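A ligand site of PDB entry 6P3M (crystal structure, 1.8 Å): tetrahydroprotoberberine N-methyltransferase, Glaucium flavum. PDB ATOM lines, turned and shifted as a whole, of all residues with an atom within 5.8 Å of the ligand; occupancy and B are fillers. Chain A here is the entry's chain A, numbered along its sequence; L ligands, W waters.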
ATOM      1  N   ILE A 121      32.002  -0.997  -3.338  1.00  0.00           N
ATOM      2  CA  ILE A 121      31.543  -0.960  -4.722  1.00  0.00           C
ATOM      3  C   ILE A 121      30.919   0.401  -5.045  1.00  0.00           C
ATOM      4  O   ILE A 121      29.869   0.506  -5.678  1.00  0.00           O
ATOM      5  CB  ILE A 121      30.596  -2.140  -5.061  1.00  0.00           C
ATOM      6  CG1 ILE A 121      30.982  -3.428  -4.333  1.00  0.00           C
ATOM      7  CG2 ILE A 121      30.560  -2.356  -6.569  1.00  0.00           C
ATOM      8  CD1 ILE A 121      30.024  -4.578  -4.634  1.00  0.00           C
ATOM      9  N   LYS A 122      31.597   1.469  -4.620  1.00  0.00           N
ATOM     10  CA  LYS A 122      31.148   2.814  -4.966  1.00  0.00           C
ATOM     11  C   LYS A 122      31.351   3.019  -6.478  1.00  0.00           C
ATOM     12  O   LYS A 122      32.386   2.690  -7.031  1.00  0.00           O
ATOM     13  CB  LYS A 122      31.968   3.825  -4.167  1.00  0.00           C
ATOM     14  CG  LYS A 122      31.479   5.260  -4.255  1.00  0.00           C
ATOM     15  CD  LYS A 122      32.128   6.098  -3.137  1.00  0.00           C
ATOM     16  CE  LYS A 122      31.496   7.467  -3.055  1.00  0.00           C
ATOM     17  NZ  LYS A 122      31.839   8.286  -4.248  1.00  0.00           N
ATOM     18  N   GLN A 123      30.328   3.593  -7.132  1.00  0.00           N
ATOM     19  CA  GLN A 123      30.341   3.769  -8.580  1.00  0.00           C
ATOM     20  C   GLN A 123      30.102   5.246  -8.872  1.00  0.00           C
ATOM     21  O   GLN A 123      29.141   5.617  -9.556  1.00  0.00           O
ATOM     22  CB  GLN A 123      29.221   2.933  -9.184  1.00  0.00           C
ATOM     23  CG  GLN A 123      29.547   1.435  -9.124  1.00  0.00           C
ATOM     24  CD  GLN A 123      28.392   0.552  -9.566  1.00  0.00           C
ATOM     25  OE1 GLN A 123      27.243   0.817  -9.256  1.00  0.00           O
ATOM     26  NE2 GLN A 123      28.713  -0.528 -10.255  1.00  0.00           N
ATOM     27  N   SER A 124      30.934   6.085  -8.250  1.00  0.00           N
ATOM     28  CA  SER A 124      30.890   7.533  -8.371  1.00  0.00           C
ATOM     29  C   SER A 124      32.300   7.980  -8.044  1.00  0.00           C
ATOM     30  O   SER A 124      33.073   7.206  -7.478  1.00  0.00           O
ATOM     31  CB  SER A 124      29.884   8.144  -7.409  1.00  0.00           C
ATOM     32  OG  SER A 124      30.008   7.600  -6.098  1.00  0.00           O
ATOM     33  N   TYR A 146      30.707  13.876   1.728  1.00  0.00           N
ATOM     34  CA  TYR A 146      29.267  14.040   1.568  1.00  0.00           C
ATOM     35  C   TYR A 146      28.587  14.292   2.917  1.00  0.00           C
ATOM     36  O   TYR A 146      27.704  15.144   3.004  1.00  0.00           O
ATOM     37  CB  TYR A 146      28.620  12.806   0.918  1.00  0.00           C
ATOM     38  CG  TYR A 146      29.236  12.327  -0.377  1.00  0.00           C
ATOM     39  CD1 TYR A 146      29.797  13.213  -1.294  1.00  0.00           C
ATOM     40  CD2 TYR A 146      29.144  10.986  -0.736  1.00  0.00           C
ATOM     41  CE1 TYR A 146      30.353  12.767  -2.484  1.00  0.00           C
ATOM     42  CE2 TYR A 146      29.685  10.532  -1.926  1.00  0.00           C
ATOM     43  CZ  TYR A 146      30.293  11.416  -2.800  1.00  0.00           C
ATOM     44  OH  TYR A 146      30.801  10.904  -3.967  1.00  0.00           O
ATOM     45  N   ASP A 160      18.783   8.215   0.295  1.00  0.00           N
ATOM     46  CA  ASP A 160      19.847   8.205  -0.704  1.00  0.00           C
ATOM     47  C   ASP A 160      19.247   7.752  -2.025  1.00  0.00           C
ATOM     48  O   ASP A 160      18.908   6.574  -2.181  1.00  0.00           O
ATOM     49  CB  ASP A 160      21.009   7.286  -0.303  1.00  0.00           C
ATOM     50  CG  ASP A 160      22.194   7.355  -1.272  1.00  0.00           C
ATOM     51  OD1 ASP A 160      22.111   8.125  -2.232  1.00  0.00           O
ATOM     52  OD2 ASP A 160      23.213   6.656  -1.052  1.00  0.00           O
ATOM     53  N   ILE A 161      19.145   8.683  -2.975  1.00  0.00           N
ATOM     54  CA  ILE A 161      18.400   8.448  -4.219  1.00  0.00           C
ATOM     55  C   ILE A 161      19.333   7.877  -5.281  1.00  0.00           C
ATOM     56  O   ILE A 161      20.337   8.510  -5.653  1.00  0.00           O
ATOM     57  CB  ILE A 161      17.690   9.731  -4.696  1.00  0.00           C
ATOM     58  CG1 ILE A 161      16.553  10.103  -3.741  1.00  0.00           C
ATOM     59  CG2 ILE A 161      17.151   9.523  -6.117  1.00  0.00           C
ATOM     60  CD1 ILE A 161      15.744  11.302  -4.160  1.00  0.00           C
ATOM     61  N   GLY A 162      18.999   6.695  -5.793  1.00  0.00           N
ATOM     62  CA  GLY A 162      19.917   5.993  -6.679  1.00  0.00           C
ATOM     63  C   GLY A 162      21.163   5.529  -5.919  1.00  0.00           C
ATOM     64  O   GLY A 162      22.294   5.858  -6.306  1.00  0.00           O
ATOM     65  N   CYS A 163      20.951   4.740  -4.853  1.00  0.00           N
ATOM     66  CA  CYS A 163      21.979   4.444  -3.857  1.00  0.00           C
ATOM     67  C   CYS A 163      23.001   3.413  -4.348  1.00  0.00           C
ATOM     68  O   CYS A 163      23.971   3.130  -3.645  1.00  0.00           O
ATOM     69  CB  CYS A 163      21.338   3.972  -2.553  1.00  0.00           C
ATOM     70  SG  CYS A 163      20.302   2.491  -2.779  1.00  0.00           S
ATOM     71  N   GLY A 164      22.793   2.804  -5.526  1.00  0.00           N
ATOM     72  CA  GLY A 164      23.784   1.874  -6.046  1.00  0.00           C
ATOM     73  C   GLY A 164      23.959   0.663  -5.127  1.00  0.00           C
ATOM     74  O   GLY A 164      22.957   0.104  -4.670  1.00  0.00           O
ATOM     75  N   GLN A 165      25.208   0.305  -4.841  1.00  0.00           N
ATOM     76  CA  GLN A 165      25.488  -0.844  -3.983  1.00  0.00           C
ATOM     77  C   GLN A 165      25.466  -0.444  -2.511  1.00  0.00           C
ATOM     78  O   GLN A 165      25.828  -1.260  -1.650  1.00  0.00           O
ATOM     79  CB  GLN A 165      26.815  -1.503  -4.349  1.00  0.00           C
ATOM     80  CG  GLN A 165      26.933  -1.897  -5.817  1.00  0.00           C
ATOM     81  CD  GLN A 165      26.053  -3.054  -6.241  1.00  0.00           C
ATOM     82  OE1 GLN A 165      25.598  -3.099  -7.385  1.00  0.00           O
ATOM     83  NE2 GLN A 165      25.832  -4.012  -5.353  1.00  0.00           N
ATOM     84  N   LEU A 184      17.220   4.202  -2.059  1.00  0.00           N
ATOM     85  CA  LEU A 184      16.238   3.972  -3.114  1.00  0.00           C
ATOM     86  C   LEU A 184      17.004   3.613  -4.386  1.00  0.00           C
ATOM     87  O   LEU A 184      17.908   4.332  -4.800  1.00  0.00           O
ATOM     88  CB  LEU A 184      15.364   5.221  -3.301  1.00  0.00           C
ATOM     89  CG  LEU A 184      14.175   5.086  -4.269  1.00  0.00           C
ATOM     90  CD1 LEU A 184      13.091   6.113  -3.969  1.00  0.00           C
ATOM     91  CD2 LEU A 184      14.616   5.211  -5.719  1.00  0.00           C
ATOM     92  N   THR A 185      16.651   2.456  -4.953  1.00  0.00           N
ATOM     93  CA  THR A 185      17.294   1.975  -6.170  1.00  0.00           C
ATOM     94  C   THR A 185      16.250   1.256  -7.023  1.00  0.00           C
ATOM     95  O   THR A 185      15.251   0.761  -6.509  1.00  0.00           O
ATOM     96  CB  THR A 185      18.460   1.017  -5.864  1.00  0.00           C
ATOM     97  OG1 THR A 185      18.940   0.530  -7.117  1.00  0.00           O
ATOM     98  CG2 THR A 185      18.062  -0.157  -4.995  1.00  0.00           C
ATOM     99  N   ASN A 186      16.505   1.215  -8.335  1.00  0.00           N
ATOM    100  CA  ASN A 186      15.585   0.568  -9.257  1.00  0.00           C
ATOM    101  C   ASN A 186      16.033  -0.859  -9.540  1.00  0.00           C
ATOM    102  O   ASN A 186      15.428  -1.556 -10.367  1.00  0.00           O
ATOM    103  CB  ASN A 186      15.478   1.375 -10.556  1.00  0.00           C
ATOM    104  CG  ASN A 186      16.784   1.542 -11.293  1.00  0.00           C
ATOM    105  OD1 ASN A 186      17.857   1.211 -10.783  1.00  0.00           O
ATOM    106  ND2 ASN A 186      16.722   2.081 -12.502  1.00  0.00           N
ATOM    107  N   GLN A 190      20.628  -4.829  -6.365  1.00  0.00           N
ATOM    108  CA  GLN A 190      21.283  -3.879  -5.483  1.00  0.00           C
ATOM    109  C   GLN A 190      20.588  -3.847  -4.121  1.00  0.00           C
ATOM    110  O   GLN A 190      21.268  -3.799  -3.097  1.00  0.00           O
ATOM    111  CB  GLN A 190      21.309  -2.478  -6.102  1.00  0.00           C
ATOM    112  CG  GLN A 190      22.235  -2.439  -7.314  1.00  0.00           C
ATOM    113  CD  GLN A 190      22.427  -1.072  -7.907  1.00  0.00           C
ATOM    114  OE1 GLN A 190      23.509  -0.759  -8.430  1.00  0.00           O
ATOM    115  NE2 GLN A 190      21.402  -0.227  -7.829  1.00  0.00           N
ATOM    116  N   ALA A 211      12.342   1.053  -6.413  1.00  0.00           N
ATOM    117  CA  ALA A 211      11.457   1.934  -7.159  1.00  0.00           C
ATOM    118  C   ALA A 211      12.249   2.615  -8.276  1.00  0.00           C
ATOM    119  O   ALA A 211      13.443   2.873  -8.135  1.00  0.00           O
ATOM    120  CB  ALA A 211      10.831   2.975  -6.253  1.00  0.00           C
ATOM    121  N   ASP A 212      11.561   2.864  -9.394  1.00  0.00           N
ATOM    122  CA  ASP A 212      11.982   3.881 -10.342  1.00  0.00           C
ATOM    123  C   ASP A 212      11.608   5.219  -9.713  1.00  0.00           C
ATOM    124  O   ASP A 212      10.426   5.484  -9.474  1.00  0.00           O
ATOM    125  CB  ASP A 212      11.265   3.645 -11.678  1.00  0.00           C
ATOM    126  CG  ASP A 212      11.418   4.737 -12.721  1.00  0.00           C
ATOM    127  OD1 ASP A 212      11.928   5.832 -12.388  1.00  0.00           O
ATOM    128  OD2 ASP A 212      11.011   4.491 -13.867  1.00  0.00           O
ATOM    129  N   VAL A 213      12.614   6.061  -9.418  1.00  0.00           N
ATOM    130  CA  VAL A 213      12.366   7.256  -8.636  1.00  0.00           C
ATOM    131  C   VAL A 213      11.393   8.187  -9.364  1.00  0.00           C
ATOM    132  O   VAL A 213      10.719   8.989  -8.719  1.00  0.00           O
ATOM    133  CB  VAL A 213      13.669   8.008  -8.305  1.00  0.00           C
ATOM    134  CG1 VAL A 213      14.294   8.658  -9.531  1.00  0.00           C
ATOM    135  CG2 VAL A 213      13.443   9.019  -7.190  1.00  0.00           C
ATOM    136  N   THR A 214      11.377   8.120 -10.704  1.00  0.00           N
ATOM    137  CA  THR A 214      10.532   9.012 -11.494  1.00  0.00           C
ATOM    138  C   THR A 214       9.054   8.654 -11.322  1.00  0.00           C
ATOM    139  O   THR A 214       8.178   9.466 -11.637  1.00  0.00           O
ATOM    140  CB  THR A 214      10.939   9.058 -12.977  1.00  0.00           C
ATOM    141  OG1 THR A 214      10.687   7.804 -13.615  1.00  0.00           O
ATOM    142  CG2 THR A 214      12.374   9.458 -13.215  1.00  0.00           C
ATOM    143  N   ILE A 228      23.792  11.167  -5.330  1.00  0.00           N
ATOM    144  CA  ILE A 228      25.206  11.114  -5.674  1.00  0.00           C
ATOM    145  C   ILE A 228      25.334  10.526  -7.092  1.00  0.00           C
ATOM    146  O   ILE A 228      25.172   9.331  -7.296  1.00  0.00           O
ATOM    147  CB  ILE A 228      26.020  10.284  -4.640  1.00  0.00           C
ATOM    148  CG1 ILE A 228      25.775  10.750  -3.200  1.00  0.00           C
ATOM    149  CG2 ILE A 228      27.494  10.313  -4.995  1.00  0.00           C
ATOM    150  CD1 ILE A 228      26.111  12.223  -2.912  1.00  0.00           C
ATOM    151  N   GLU A 229      25.588  11.405  -8.067  1.00  0.00           N
ATOM    152  CA  GLU A 229      25.767  11.019  -9.467  1.00  0.00           C
ATOM    153  C   GLU A 229      24.589  10.203 -10.017  1.00  0.00           C
ATOM    154  O   GLU A 229      24.770   9.301 -10.835  1.00  0.00           O
ATOM    155  CB  GLU A 229      27.169  10.425  -9.666  1.00  0.00           C
ATOM    156  CG  GLU A 229      28.232  11.507  -9.426  1.00  0.00           C
ATOM    157  CD  GLU A 229      29.691  11.111  -9.344  1.00  0.00           C
ATOM    158  OE1 GLU A 229      30.470  11.796  -8.640  1.00  0.00           O
ATOM    159  OE2 GLU A 229      30.065  10.136 -10.017  1.00  0.00           O
ATOM    160  N   THR A 230      23.372  10.563  -9.590  1.00  0.00           N
ATOM    161  CA  THR A 230      22.142   9.966 -10.099  1.00  0.00           C
ATOM    162  C   THR A 230      21.448  10.935 -11.063  1.00  0.00           C
ATOM    163  O   THR A 230      20.805  10.516 -12.008  1.00  0.00           O
ATOM    164  CB  THR A 230      21.243   9.530  -8.933  1.00  0.00           C
ATOM    165  OG1 THR A 230      22.036   8.521  -8.298  1.00  0.00           O
ATOM    166  CG2 THR A 230      19.931   8.924  -9.389  1.00  0.00           C
ATOM    167  N   HIS A 233      21.311  10.805 -14.837  1.00  0.00           N
ATOM    168  CA  HIS A 233      20.497   9.794 -15.497  1.00  0.00           C
ATOM    169  C   HIS A 233      19.045  10.261 -15.652  1.00  0.00           C
ATOM    170  O   HIS A 233      18.194   9.522 -16.135  1.00  0.00           O
ATOM    171  CB  HIS A 233      20.594   8.442 -14.745  1.00  0.00           C
ATOM    172  CG  HIS A 233      21.982   7.902 -14.715  1.00  0.00           C
ATOM    173  ND1 HIS A 233      22.507   7.182 -15.769  1.00  0.00           N
ATOM    174  CD2 HIS A 233      22.981   8.070 -13.815  1.00  0.00           C
ATOM    175  CE1 HIS A 233      23.769   6.886 -15.507  1.00  0.00           C
ATOM    176  NE2 HIS A 233      24.087   7.428 -14.311  1.00  0.00           N
ATOM    177  N   MET A 234      18.767  11.516 -15.268  1.00  0.00           N
ATOM    178  CA  MET A 234      17.383  11.951 -15.140  1.00  0.00           C
ATOM    179  C   MET A 234      16.897  12.618 -16.410  1.00  0.00           C
ATOM    180  O   MET A 234      17.520  13.562 -16.909  1.00  0.00           O
ATOM    181  CB  MET A 234      17.173  12.886 -13.949  1.00  0.00           C
ATOM    182  CG  MET A 234      17.177  12.110 -12.661  1.00  0.00           C
ATOM    183  SD  MET A 234      15.930  10.787 -12.710  1.00  0.00           S
ATOM    184  CE  MET A 234      16.946   9.344 -12.409  1.00  0.00           C
HETATM  185  N1  LIG L   1      24.894   6.790  -5.726  1.00  0.00           N
HETATM  186  C1  LIG L   1      25.592   5.484  -6.054  1.00  0.00           C
HETATM  187  C2  LIG L   1      25.257   5.033  -7.482  1.00  0.00           C
HETATM  188  C3  LIG L   1      25.595   6.092  -8.510  1.00  0.00           C
HETATM  189  S1  LIG L   1      25.224   5.546 -10.212  1.00  0.00           S
HETATM  190  C4  LIG L   1      27.106   5.645  -5.925  1.00  0.00           C
HETATM  191  O1  LIG L   1      27.591   6.764  -5.701  1.00  0.00           O
HETATM  192  O2  LIG L   1      27.874   4.657  -6.066  1.00  0.00           O
HETATM  193  C5  LIG L   1      23.523   6.136 -10.424  1.00  0.00           C
HETATM  194  C6  LIG L   1      22.564   5.149  -9.826  1.00  0.00           C
HETATM  195  O3  LIG L   1      21.190   5.595  -9.985  1.00  0.00           O
HETATM  196  C7  LIG L   1      22.634   3.774 -10.495  1.00  0.00           C
HETATM  197  O4  LIG L   1      22.489   2.762  -9.522  1.00  0.00           O
HETATM  198  C8  LIG L   1      21.421   3.809 -11.418  1.00  0.00           C
HETATM  199  O5  LIG L   1      21.005   2.538 -11.862  1.00  0.00           O
HETATM  200  C9  LIG L   1      20.437   4.496 -10.468  1.00  0.00           C
HETATM  201  N2  LIG L   1      19.238   4.960 -11.160  1.00  0.00           N
HETATM  202  C10 LIG L   1      19.203   5.475 -12.433  1.00  0.00           C
HETATM  203  N3  LIG L   1      17.994   5.832 -12.815  1.00  0.00           N
HETATM  204  C11 LIG L   1      17.186   5.531 -11.723  1.00  0.00           C
HETATM  205  C12 LIG L   1      15.801   5.662 -11.509  1.00  0.00           C
HETATM  206  N4  LIG L   1      14.963   6.182 -12.401  1.00  0.00           N
HETATM  207  N5  LIG L   1      15.311   5.232 -10.316  1.00  0.00           N
HETATM  208  C13 LIG L   1      16.162   4.747  -9.405  1.00  0.00           C
HETATM  209  N6  LIG L   1      17.483   4.573  -9.513  1.00  0.00           N
HETATM  210  C14 LIG L   1      17.939   4.983 -10.698  1.00  0.00           C
HETATM  211  O   HOH W   1      22.825   8.696  -4.607  1.00  0.00           O
HETATM  212  O   HOH W   2      24.767   1.192 -10.047  1.00  0.00           O
HETATM  213  O   HOH W   3      27.338   2.099  -5.650  1.00  0.00           O
HETATM  214  O   HOH W   4      19.300   2.302 -14.031  1.00  0.00           O
HETATM  215  O   HOH W   5      20.573   0.433 -10.442  1.00  0.00           O
HETATM  216  O   HOH W   6      27.924   7.241  -2.821  1.00  0.00           O
HETATM  217  O   HOH W   7      25.143   7.054  -2.963  1.00  0.00           O
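OG1 of Thr 230 is in hydrogen-bond range of O3 of the ligand (3.5 Å). O of Ile 228 lies within hydrogen-bond range of N1 of the ligand, at 3.0 Å. The side-chain carboxylate (OD1) of Asp 212 lies within hydrogen-bond range of a nitrogen (N4) of the ligand (3.1 Å). The backbone NH (N) of Gln 123 lies within hydrogen-bond range of an oxygen (O2) of the ligand (2.9 Å). N of Val 213 lies within hydrogen-bond range of N5 of the ligand. OG of Ser 124 lies within hydrogen-bond range of O1 of the ligand. N1 of the ligand sits at hydrogen-bond distance from O of Gly 162 (2.8 Å).
The backbone carbonyl oxygen (O) of Ile 161 sits at hydrogen-bond distance from the side-chain hydroxyl (OG1) of Thr 230 (3.1 Å). The side-chain amino group (NZ) of Lys 122 lies within hydrogen-bond range of the side-chain hydroxyl (OH) of Tyr 146. The side-chain amide nitrogen (NE2) of Gln 190 lies within hydrogen-bond range of the side-chain hydroxyl (OG1) of Thr 185 (2.7 Å). OG1 of Thr 214 sits at hydrogen-bond distance from OD1 of Asp 212, 2.6 Å away. N of Gly 162 is in hydrogen-bond range of O of Leu 184 (2.8 Å). The side-chain hydroxyl (OG) of Ser 124 lies within hydrogen-bond range of the side-chain amino group (NZ) of Lys 122 (2.7 Å). The backbone carbonyl oxygen of Thr 185 sits at hydrogen-bond distance from the backbone NH of Ala 211 (2.9 Å). The side-chain hydroxyl (OG1) of Thr 230 lies within hydrogen-bond range of the backbone carbonyl oxygen (O) of Gly 162.
Residues that only touch the ligand: Glu 229, Ala 211, Asn 186, Gln 190, Met 234, Cys 163, Gly 164, Lys 122 and His 233. Hydrophobic or aromatic side chains within 4 Å of the ligand: Val 213, Ile 228, His 233 and Met 234. Within 4 Å of the ligand: Lys 122, Gln 123, Ser 124, Gly 162, Cys 163, Gly 164, Asn 186, Gln 190, Ala 211, Asp 212, Val 213, Ile 228, Glu 229, Thr 230, His 233 and Met 234. The nearest printed residue that does not touch the ligand is Leu 184 (4.02 Å).
Water W5 lies within hydrogen-bond range of O5 of the ligand, NE2 of Gln 190 and OD1 of Asn 186. Water W3 lies within hydrogen-bond range of an oxygen (O2) of the ligand (2.6 Å), the backbone NH of Gln 165 (2.9 Å) and the backbone carbonyl oxygen of Ile 121 (3.0 Å). Water W4 bridges O5 of the ligand (2.8 Å) and ND2 of Asn 186 (3.0 Å). Water W7 bridges OD2 of Asp 160 and N1 of the ligand. Water W2 lies within hydrogen-bond range of OE1 of Gln 123 (2.6 Å), O4 of the ligand (2.8 Å) and OE1 of Gln 190 (2.8 Å).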
